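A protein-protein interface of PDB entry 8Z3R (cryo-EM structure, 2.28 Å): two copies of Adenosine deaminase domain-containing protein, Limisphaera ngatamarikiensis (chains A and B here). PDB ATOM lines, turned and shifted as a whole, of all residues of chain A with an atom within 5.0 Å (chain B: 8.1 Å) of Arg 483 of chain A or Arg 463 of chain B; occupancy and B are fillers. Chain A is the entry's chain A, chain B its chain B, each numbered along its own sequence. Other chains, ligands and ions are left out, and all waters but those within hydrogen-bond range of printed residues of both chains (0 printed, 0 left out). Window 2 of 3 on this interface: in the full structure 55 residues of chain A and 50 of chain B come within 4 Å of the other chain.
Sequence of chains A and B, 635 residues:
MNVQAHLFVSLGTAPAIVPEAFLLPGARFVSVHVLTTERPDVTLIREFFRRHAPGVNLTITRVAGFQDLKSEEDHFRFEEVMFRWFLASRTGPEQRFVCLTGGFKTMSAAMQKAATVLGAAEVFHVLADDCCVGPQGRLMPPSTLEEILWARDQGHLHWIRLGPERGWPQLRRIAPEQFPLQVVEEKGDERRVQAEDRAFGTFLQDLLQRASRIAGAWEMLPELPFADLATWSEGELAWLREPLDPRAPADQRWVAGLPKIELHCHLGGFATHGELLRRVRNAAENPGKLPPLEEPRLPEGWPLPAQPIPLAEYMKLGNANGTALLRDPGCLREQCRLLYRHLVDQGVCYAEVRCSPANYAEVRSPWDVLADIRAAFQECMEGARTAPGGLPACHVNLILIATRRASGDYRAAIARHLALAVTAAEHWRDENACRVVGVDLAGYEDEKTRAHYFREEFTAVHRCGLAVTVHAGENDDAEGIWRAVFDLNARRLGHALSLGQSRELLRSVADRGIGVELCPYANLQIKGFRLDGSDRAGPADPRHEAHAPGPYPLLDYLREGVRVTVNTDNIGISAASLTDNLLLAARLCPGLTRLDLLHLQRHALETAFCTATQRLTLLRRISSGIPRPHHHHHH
OE2 of Glu 479 of chain A lies within salt-bridge range of NH2 of Arg 463 of chain B (3.2 Å).
The side-chain carboxylate of Asp 487 of chain A lies within salt-bridge range of the guanidinium group of Arg 455 of chain B (3.4 Å).
The backbone carbonyl oxygen (O) of Phe 486 of chain A lies close to the side-chain amide oxygen (OD1) of Asn 489 of chain B (3.2 Å).
O of Ala 460 of chain B is in hydrogen-bond range of SG of Cys 464 of chain B.
NE of Arg 483 of chain A is in salt-bridge range of OE2 of Glu 479 of chain A (3.4 Å).
The side-chain carboxylate (OD1) of Asp 487 of chain A lies within salt-bridge range of the guanidinium group (NH1) of Arg 483 of chain A (3.3 Å).
The backbone carbonyl oxygen of Arg 483 of chain A sits at hydrogen-bond distance from the backbone NH of Leu 488 of chain A (3.5 Å).
Among the printed residues, pairs that only touch across the chains: Phe 486 of chain A with His 462 of chain B (3.4 Å), Trp 482 of chain A with Arg 463 of chain B (3.5 Å), Glu 504 of chain A with Cys 464 of chain B (3.9 Å), Arg 483 of chain A with Arg 463 of chain B (3.9 Å), Phe 486 of chain A with Arg 455 of chain B (3.96 Å) and Trp 482 of chain A with His 462 of chain B (3.97 Å).
Of the printed residues of chain B, Glu 479 of chain A touches Arg 463.
Val 485 of chain A touches none of the printed residues of chain B.
Of the printed residues of chain B, Asp 487 of chain A touches Arg 455.
Of the printed residues of chain A, Arg 455 of chain B touches Phe 486 (3.96 Å) and Asp 487 (3.4 Å).
Arg 463 of chain B touches just these residues of chain A: Glu 479, Trp 482 and Arg 483.
Of the printed residues of chain A, Cys 464 of chain B touches Glu 504 (3.9 Å).
The nearest printed residue of chain B that does not touch Trp 482 of chain A is Thr 459 of chain B (4.6 Å).
Printed residues of chain B that touch a printed residue of chain A: Arg 455, His 462, Arg 463, Cys 464 and Asn 489.
Hydrophobic or aromatic side chains of chain B within 4 Å of the printed part of chain A: His 462.
Printed residues of chain A that touch a printed residue of chain B: Glu 479, Trp 482, Arg 483, Phe 486, Asp 487 and Glu 504.
No position is printed for both chains.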
ATOM      1  N   ALA A 451      16.173  20.206  11.170  1.00  0.00           N
ATOM      2  CA  ALA A 451      16.077  21.653  11.337  1.00  0.00           C
ATOM      3  C   ALA A 451      14.659  22.161  11.111  1.00  0.00           C
ATOM      4  O   ALA A 451      14.229  23.119  11.764  1.00  0.00           O
ATOM      5  CB  ALA A 451      17.052  22.352  10.390  1.00  0.00           C
ATOM      6  N   HIS A 452      13.914  21.539  10.197  1.00  0.00           N
ATOM      7  CA  HIS A 452      12.602  22.064   9.831  1.00  0.00           C
ATOM      8  C   HIS A 452      11.559  21.890  10.928  1.00  0.00           C
ATOM      9  O   HIS A 452      10.423  22.343  10.749  1.00  0.00           O
ATOM     10  CB  HIS A 452      12.116  21.409   8.536  1.00  0.00           C
ATOM     11  CG  HIS A 452      11.918  19.929   8.638  1.00  0.00           C
ATOM     12  ND1 HIS A 452      12.900  19.023   8.300  1.00  0.00           N
ATOM     13  CD2 HIS A 452      10.850  19.196   9.031  1.00  0.00           C
ATOM     14  CE1 HIS A 452      12.448  17.796   8.491  1.00  0.00           C
ATOM     15  NE2 HIS A 452      11.206  17.874   8.932  1.00  0.00           N
ATOM     16  N   GLU A 479      19.954  15.353   3.455  1.00  0.00           N
ATOM     17  CA  GLU A 479      18.629  15.930   3.659  1.00  0.00           C
ATOM     18  C   GLU A 479      18.628  16.912   4.825  1.00  0.00           C
ATOM     19  O   GLU A 479      17.974  17.960   4.763  1.00  0.00           O
ATOM     20  CB  GLU A 479      17.600  14.823   3.884  1.00  0.00           C
ATOM     21  CG  GLU A 479      16.189  15.328   4.149  1.00  0.00           C
ATOM     22  CD  GLU A 479      15.480  15.800   2.891  1.00  0.00           C
ATOM     23  OE1 GLU A 479      16.091  15.760   1.803  1.00  0.00           O
ATOM     24  OE2 GLU A 479      14.307  16.214   2.993  1.00  0.00           O
ATOM     25  N   GLY A 480      19.351  16.588   5.898  1.00  0.00           N
ATOM     26  CA  GLY A 480      19.452  17.516   7.013  1.00  0.00           C
ATOM     27  C   GLY A 480      20.120  18.820   6.625  1.00  0.00           C
ATOM     28  O   GLY A 480      19.685  19.898   7.039  1.00  0.00           O
ATOM     29  N   ILE A 481      21.178  18.742   5.816  1.00  0.00           N
ATOM     30  CA  ILE A 481      21.851  19.949   5.346  1.00  0.00           C
ATOM     31  C   ILE A 481      20.916  20.770   4.467  1.00  0.00           C
ATOM     32  O   ILE A 481      20.857  22.001   4.579  1.00  0.00           O
ATOM     33  CB  ILE A 481      23.151  19.584   4.605  1.00  0.00           C
ATOM     34  CG1 ILE A 481      24.151  18.948   5.568  1.00  0.00           C
ATOM     35  CG2 ILE A 481      23.762  20.815   3.961  1.00  0.00           C
ATOM     36  CD1 ILE A 481      25.074  17.949   4.915  1.00  0.00           C
ATOM     37  N   TRP A 482      20.174  20.104   3.578  1.00  0.00           N
ATOM     38  CA  TRP A 482      19.228  20.816   2.726  1.00  0.00           C
ATOM     39  C   TRP A 482      18.163  21.523   3.553  1.00  0.00           C
ATOM     40  O   TRP A 482      17.818  22.680   3.280  1.00  0.00           O
ATOM     41  CB  TRP A 482      18.580  19.848   1.735  1.00  0.00           C
ATOM     42  CG  TRP A 482      17.777  20.524   0.661  1.00  0.00           C
ATOM     43  CD1 TRP A 482      18.193  20.830  -0.600  1.00  0.00           C
ATOM     44  CD2 TRP A 482      16.416  20.966   0.752  1.00  0.00           C
ATOM     45  NE1 TRP A 482      17.181  21.440  -1.299  1.00  0.00           N
ATOM     46  CE2 TRP A 482      16.078  21.535  -0.491  1.00  0.00           C
ATOM     47  CE3 TRP A 482      15.451  20.937   1.764  1.00  0.00           C
ATOM     48  CZ2 TRP A 482      14.820  22.072  -0.749  1.00  0.00           C
ATOM     49  CZ3 TRP A 482      14.204  21.471   1.506  1.00  0.00           C
ATOM     50  CH2 TRP A 482      13.898  22.030   0.260  1.00  0.00           C
ATOM     51  N   ARG A 483      17.623  20.839   4.563  1.00  0.00           N
ATOM     52  CA  ARG A 483      16.609  21.457   5.410  1.00  0.00           C
ATOM     53  C   ARG A 483      17.177  22.622   6.209  1.00  0.00           C
ATOM     54  O   ARG A 483      16.512  23.653   6.348  1.00  0.00           O
ATOM     55  CB  ARG A 483      15.991  20.417   6.341  1.00  0.00           C
ATOM     56  CG  ARG A 483      15.202  19.349   5.613  1.00  0.00           C
ATOM     57  CD  ARG A 483      13.783  19.809   5.338  1.00  0.00           C
ATOM     58  NE  ARG A 483      12.965  18.745   4.774  1.00  0.00           N
ATOM     59  CZ  ARG A 483      11.755  18.923   4.262  1.00  0.00           C
ATOM     60  NH1 ARG A 483      11.185  20.116   4.234  1.00  0.00           N
ATOM     61  NH2 ARG A 483      11.099  17.878   3.767  1.00  0.00           N
ATOM     62  N   ALA A 484      18.400  22.488   6.724  1.00  0.00           N
ATOM     63  CA  ALA A 484      19.020  23.597   7.440  1.00  0.00           C
ATOM     64  C   ALA A 484      19.225  24.796   6.526  1.00  0.00           C
ATOM     65  O   ALA A 484      19.018  25.944   6.938  1.00  0.00           O
ATOM     66  CB  ALA A 484      20.347  23.151   8.049  1.00  0.00           C
ATOM     67  N   VAL A 485      19.637  24.552   5.282  1.00  0.00           N
ATOM     68  CA  VAL A 485      19.917  25.649   4.362  1.00  0.00           C
ATOM     69  C   VAL A 485      18.631  26.346   3.932  1.00  0.00           C
ATOM     70  O   VAL A 485      18.558  27.580   3.911  1.00  0.00           O
ATOM     71  CB  VAL A 485      20.714  25.134   3.151  1.00  0.00           C
ATOM     72  CG1 VAL A 485      20.658  26.133   2.008  1.00  0.00           C
ATOM     73  CG2 VAL A 485      22.154  24.856   3.545  1.00  0.00           C
ATOM     74  N   PHE A 486      17.593  25.580   3.589  1.00  0.00           N
ATOM     75  CA  PHE A 486      16.449  26.152   2.891  1.00  0.00           C
ATOM     76  C   PHE A 486      15.226  26.387   3.769  1.00  0.00           C
ATOM     77  O   PHE A 486      14.350  27.164   3.375  1.00  0.00           O
ATOM     78  CB  PHE A 486      16.055  25.258   1.709  1.00  0.00           C
ATOM     79  CG  PHE A 486      16.816  25.558   0.451  1.00  0.00           C
ATOM     80  CD1 PHE A 486      16.596  26.734  -0.241  1.00  0.00           C
ATOM     81  CD2 PHE A 486      17.764  24.672  -0.031  1.00  0.00           C
ATOM     82  CE1 PHE A 486      17.297  27.016  -1.395  1.00  0.00           C
ATOM     83  CE2 PHE A 486      18.468  24.950  -1.184  1.00  0.00           C
ATOM     84  CZ  PHE A 486      18.234  26.123  -1.867  1.00  0.00           C
ATOM     85  N   ASP A 487      15.131  25.748   4.934  1.00  0.00           N
ATOM     86  CA  ASP A 487      13.997  25.946   5.826  1.00  0.00           C
ATOM     87  C   ASP A 487      14.331  26.761   7.063  1.00  0.00           C
ATOM     88  O   ASP A 487      13.422  27.310   7.686  1.00  0.00           O
ATOM     89  CB  ASP A 487      13.419  24.595   6.264  1.00  0.00           C
ATOM     90  CG  ASP A 487      12.534  23.969   5.206  1.00  0.00           C
ATOM     91  OD1 ASP A 487      11.708  23.101   5.556  1.00  0.00           O
ATOM     92  OD2 ASP A 487      12.665  24.344   4.023  1.00  0.00           O
ATOM     93  N   LEU A 488      15.606  26.850   7.434  1.00  0.00           N
ATOM     94  CA  LEU A 488      16.030  27.624   8.590  1.00  0.00           C
ATOM     95  C   LEU A 488      16.894  28.819   8.213  1.00  0.00           C
ATOM     96  O   LEU A 488      17.277  29.592   9.098  1.00  0.00           O
ATOM     97  CB  LEU A 488      16.782  26.724   9.578  1.00  0.00           C
ATOM     98  CG  LEU A 488      16.663  27.087  11.059  1.00  0.00           C
ATOM     99  CD1 LEU A 488      15.234  26.895  11.533  1.00  0.00           C
ATOM    100  CD2 LEU A 488      17.616  26.255  11.895  1.00  0.00           C
ATOM    101  N   GLU A 504      23.593  18.930  -6.507  1.00  0.00           N
ATOM    102  CA  GLU A 504      22.811  20.159  -6.604  1.00  0.00           C
ATOM    103  C   GLU A 504      22.913  20.982  -5.327  1.00  0.00           C
ATOM    104  O   GLU A 504      23.042  22.212  -5.378  1.00  0.00           O
ATOM    105  CB  GLU A 504      21.353  19.826  -6.916  1.00  0.00           C
ATOM    106  CG  GLU A 504      21.165  18.978  -8.160  1.00  0.00           C
ATOM    107  CD  GLU A 504      21.088  17.496  -7.852  1.00  0.00           C
ATOM    108  OE1 GLU A 504      21.424  17.101  -6.716  1.00  0.00           O
ATOM    109  OE2 GLU A 504      20.695  16.722  -8.749  1.00  0.00           O
ATOM    110  N   VAL B 422      13.128  24.333 -15.469  1.00  0.00           N
ATOM    111  CA  VAL B 422      13.918  23.235 -14.916  1.00  0.00           C
ATOM    112  C   VAL B 422      14.420  22.325 -16.033  1.00  0.00           C
ATOM    113  O   VAL B 422      15.609  21.979 -16.095  1.00  0.00           O
ATOM    114  CB  VAL B 422      13.098  22.453 -13.874  1.00  0.00           C
ATOM    115  CG1 VAL B 422      13.803  21.161 -13.504  1.00  0.00           C
ATOM    116  CG2 VAL B 422      12.865  23.303 -12.639  1.00  0.00           C
ATOM    117  N   GLU B 426      18.319  21.780 -17.332  1.00  0.00           N
ATOM    118  CA  GLU B 426      18.946  20.463 -17.395  1.00  0.00           C
ATOM    119  C   GLU B 426      19.451  20.136 -18.797  1.00  0.00           C
ATOM    120  O   GLU B 426      20.424  19.387 -18.941  1.00  0.00           O
ATOM    121  CB  GLU B 426      17.969  19.387 -16.922  1.00  0.00           C
ATOM    122  CG  GLU B 426      17.600  19.487 -15.453  1.00  0.00           C
ATOM    123  CD  GLU B 426      18.776  19.206 -14.540  1.00  0.00           C
ATOM    124  OE1 GLU B 426      19.647  18.398 -14.922  1.00  0.00           O
ATOM    125  OE2 GLU B 426      18.829  19.793 -13.439  1.00  0.00           O
ATOM    126  N   ARG B 455       5.092  29.184  -2.228  1.00  0.00           N
ATOM    127  CA  ARG B 455       6.219  28.400  -1.730  1.00  0.00           C
ATOM    128  C   ARG B 455       6.197  26.976  -2.278  1.00  0.00           C
ATOM    129  O   ARG B 455       7.239  26.437  -2.682  1.00  0.00           O
ATOM    130  CB  ARG B 455       6.197  28.398  -0.202  1.00  0.00           C
ATOM    131  CG  ARG B 455       7.363  27.699   0.467  1.00  0.00           C
ATOM    132  CD  ARG B 455       7.268  27.854   1.978  1.00  0.00           C
ATOM    133  NE  ARG B 455       8.322  27.131   2.679  1.00  0.00           N
ATOM    134  CZ  ARG B 455       9.526  27.624   2.935  1.00  0.00           C
ATOM    135  NH1 ARG B 455       9.868  28.845   2.555  1.00  0.00           N
ATOM    136  NH2 ARG B 455      10.409  26.875   3.587  1.00  0.00           N
ATOM    137  N   PHE B 458       7.628  26.748  -5.718  1.00  0.00           N
ATOM    138  CA  PHE B 458       9.066  26.936  -5.846  1.00  0.00           C
ATOM    139  C   PHE B 458       9.882  25.895  -5.091  1.00  0.00           C
ATOM    140  O   PHE B 458      11.118  25.921  -5.174  1.00  0.00           O
ATOM    141  CB  PHE B 458       9.452  28.339  -5.366  1.00  0.00           C
ATOM    142  CG  PHE B 458       9.223  29.411  -6.389  1.00  0.00           C
ATOM    143  CD1 PHE B 458       7.954  29.918  -6.606  1.00  0.00           C
ATOM    144  CD2 PHE B 458      10.274  29.910  -7.136  1.00  0.00           C
ATOM    145  CE1 PHE B 458       7.738  30.903  -7.548  1.00  0.00           C
ATOM    146  CE2 PHE B 458      10.064  30.896  -8.080  1.00  0.00           C
ATOM    147  CZ  PHE B 458       8.794  31.393  -8.286  1.00  0.00           C
ATOM    148  N   THR B 459       9.233  24.990  -4.354  1.00  0.00           N
ATOM    149  CA  THR B 459       9.990  23.940  -3.674  1.00  0.00           C
ATOM    150  C   THR B 459      10.755  23.071  -4.672  1.00  0.00           C
ATOM    151  O   THR B 459      11.903  22.689  -4.415  1.00  0.00           O
ATOM    152  CB  THR B 459       9.064  23.094  -2.793  1.00  0.00           C
ATOM    153  OG1 THR B 459       9.846  22.183  -2.010  1.00  0.00           O
ATOM    154  CG2 THR B 459       8.056  22.307  -3.620  1.00  0.00           C
ATOM    155  N   ALA B 460      10.153  22.772  -5.827  1.00  0.00           N
ATOM    156  CA  ALA B 460      10.842  21.972  -6.836  1.00  0.00           C
ATOM    157  C   ALA B 460      12.015  22.731  -7.442  1.00  0.00           C
ATOM    158  O   ALA B 460      13.077  22.148  -7.695  1.00  0.00           O
ATOM    159  CB  ALA B 460       9.861  21.541  -7.924  1.00  0.00           C
ATOM    160  N   VAL B 461      11.837  24.031  -7.690  1.00  0.00           N
ATOM    161  CA  VAL B 461      12.924  24.848  -8.222  1.00  0.00           C
ATOM    162  C   VAL B 461      14.093  24.870  -7.249  1.00  0.00           C
ATOM    163  O   VAL B 461      15.260  24.782  -7.652  1.00  0.00           O
ATOM    164  CB  VAL B 461      12.419  26.268  -8.536  1.00  0.00           C
ATOM    165  CG1 VAL B 461      13.564  27.155  -8.990  1.00  0.00           C
ATOM    166  CG2 VAL B 461      11.328  26.221  -9.591  1.00  0.00           C
ATOM    167  N   HIS B 462      13.803  24.987  -5.952  1.00  0.00           N
ATOM    168  CA  HIS B 462      14.873  24.964  -4.960  1.00  0.00           C
ATOM    169  C   HIS B 462      15.526  23.590  -4.874  1.00  0.00           C
ATOM    170  O   HIS B 462      16.742  23.489  -4.672  1.00  0.00           O
ATOM    171  CB  HIS B 462      14.339  25.396  -3.596  1.00  0.00           C
ATOM    172  CG  HIS B 462      14.024  26.856  -3.515  1.00  0.00           C
ATOM    173  ND1 HIS B 462      14.978  27.830  -3.711  1.00  0.00           N
ATOM    174  CD2 HIS B 462      12.866  27.508  -3.258  1.00  0.00           C
ATOM    175  CE1 HIS B 462      14.419  29.020  -3.584  1.00  0.00           C
ATOM    176  NE2 HIS B 462      13.139  28.853  -3.308  1.00  0.00           N
ATOM    177  N   ARG B 463      14.739  22.522  -5.019  1.00  0.00           N
ATOM    178  CA  ARG B 463      15.310  21.178  -4.987  1.00  0.00           C
ATOM    179  C   ARG B 463      16.260  20.950  -6.156  1.00  0.00           C
ATOM    180  O   ARG B 463      17.324  20.344  -5.991  1.00  0.00           O
ATOM    181  CB  ARG B 463      14.196  20.132  -4.989  1.00  0.00           C
ATOM    182  CG  ARG B 463      13.490  19.981  -3.656  1.00  0.00           C
ATOM    183  CD  ARG B 463      13.916  18.712  -2.945  1.00  0.00           C
ATOM    184  NE  ARG B 463      13.383  18.646  -1.590  1.00  0.00           N
ATOM    185  CZ  ARG B 463      14.041  18.153  -0.551  1.00  0.00           C
ATOM    186  NH1 ARG B 463      15.263  17.665  -0.675  1.00  0.00           N
ATOM    187  NH2 ARG B 463      13.456  18.146   0.642  1.00  0.00           N
ATOM    188  N   CYS B 464      15.895  21.426  -7.346  1.00  0.00           N
ATOM    189  CA  CYS B 464      16.743  21.233  -8.516  1.00  0.00           C
ATOM    190  C   CYS B 464      17.930  22.187  -8.561  1.00  0.00           C
ATOM    191  O   CYS B 464      18.876  21.934  -9.314  1.00  0.00           O
ATOM    192  CB  CYS B 464      15.917  21.379  -9.796  1.00  0.00           C
ATOM    193  SG  CYS B 464      14.661  20.098 -10.009  1.00  0.00           S
ATOM    194  N   GLY B 465      17.909  23.265  -7.782  1.00  0.00           N
ATOM    195  CA  GLY B 465      19.048  24.159  -7.699  1.00  0.00           C
ATOM    196  C   GLY B 465      19.098  25.244  -8.755  1.00  0.00           C
ATOM    197  O   GLY B 465      20.085  25.356  -9.488  1.00  0.00           O
ATOM    198  N   LEU B 466      18.045  26.052  -8.845  1.00  0.00           N
ATOM    199  CA  LEU B 466      18.005  27.197  -9.742  1.00  0.00           C
ATOM    200  C   LEU B 466      17.892  28.487  -8.941  1.00  0.00           C
ATOM    201  O   LEU B 466      17.310  28.516  -7.855  1.00  0.00           O
ATOM    202  CB  LEU B 466      16.832  27.099 -10.720  1.00  0.00           C
ATOM    203  CG  LEU B 466      16.866  25.970 -11.744  1.00  0.00           C
ATOM    204  CD1 LEU B 466      15.569  25.941 -12.533  1.00  0.00           C
ATOM    205  CD2 LEU B 466      18.054  26.138 -12.671  1.00  0.00           C
ATOM    206  N   ASN B 489      13.566  32.315  -0.496  1.00  0.00           N
ATOM    207  CA  ASN B 489      15.026  32.244  -0.553  1.00  0.00           C
ATOM    208  C   ASN B 489      15.569  32.972  -1.779  1.00  0.00           C
ATOM    209  O   ASN B 489      16.464  32.485  -2.473  1.00  0.00           O
ATOM    210  CB  ASN B 489      15.501  30.791  -0.528  1.00  0.00           C
ATOM    211  CG  ASN B 489      15.216  30.108   0.794  1.00  0.00           C
ATOM    212  OD1 ASN B 489      14.396  29.195   0.868  1.00  0.00           O
ATOM    213  ND2 ASN B 489      15.899  30.543   1.845  1.00  0.00           N
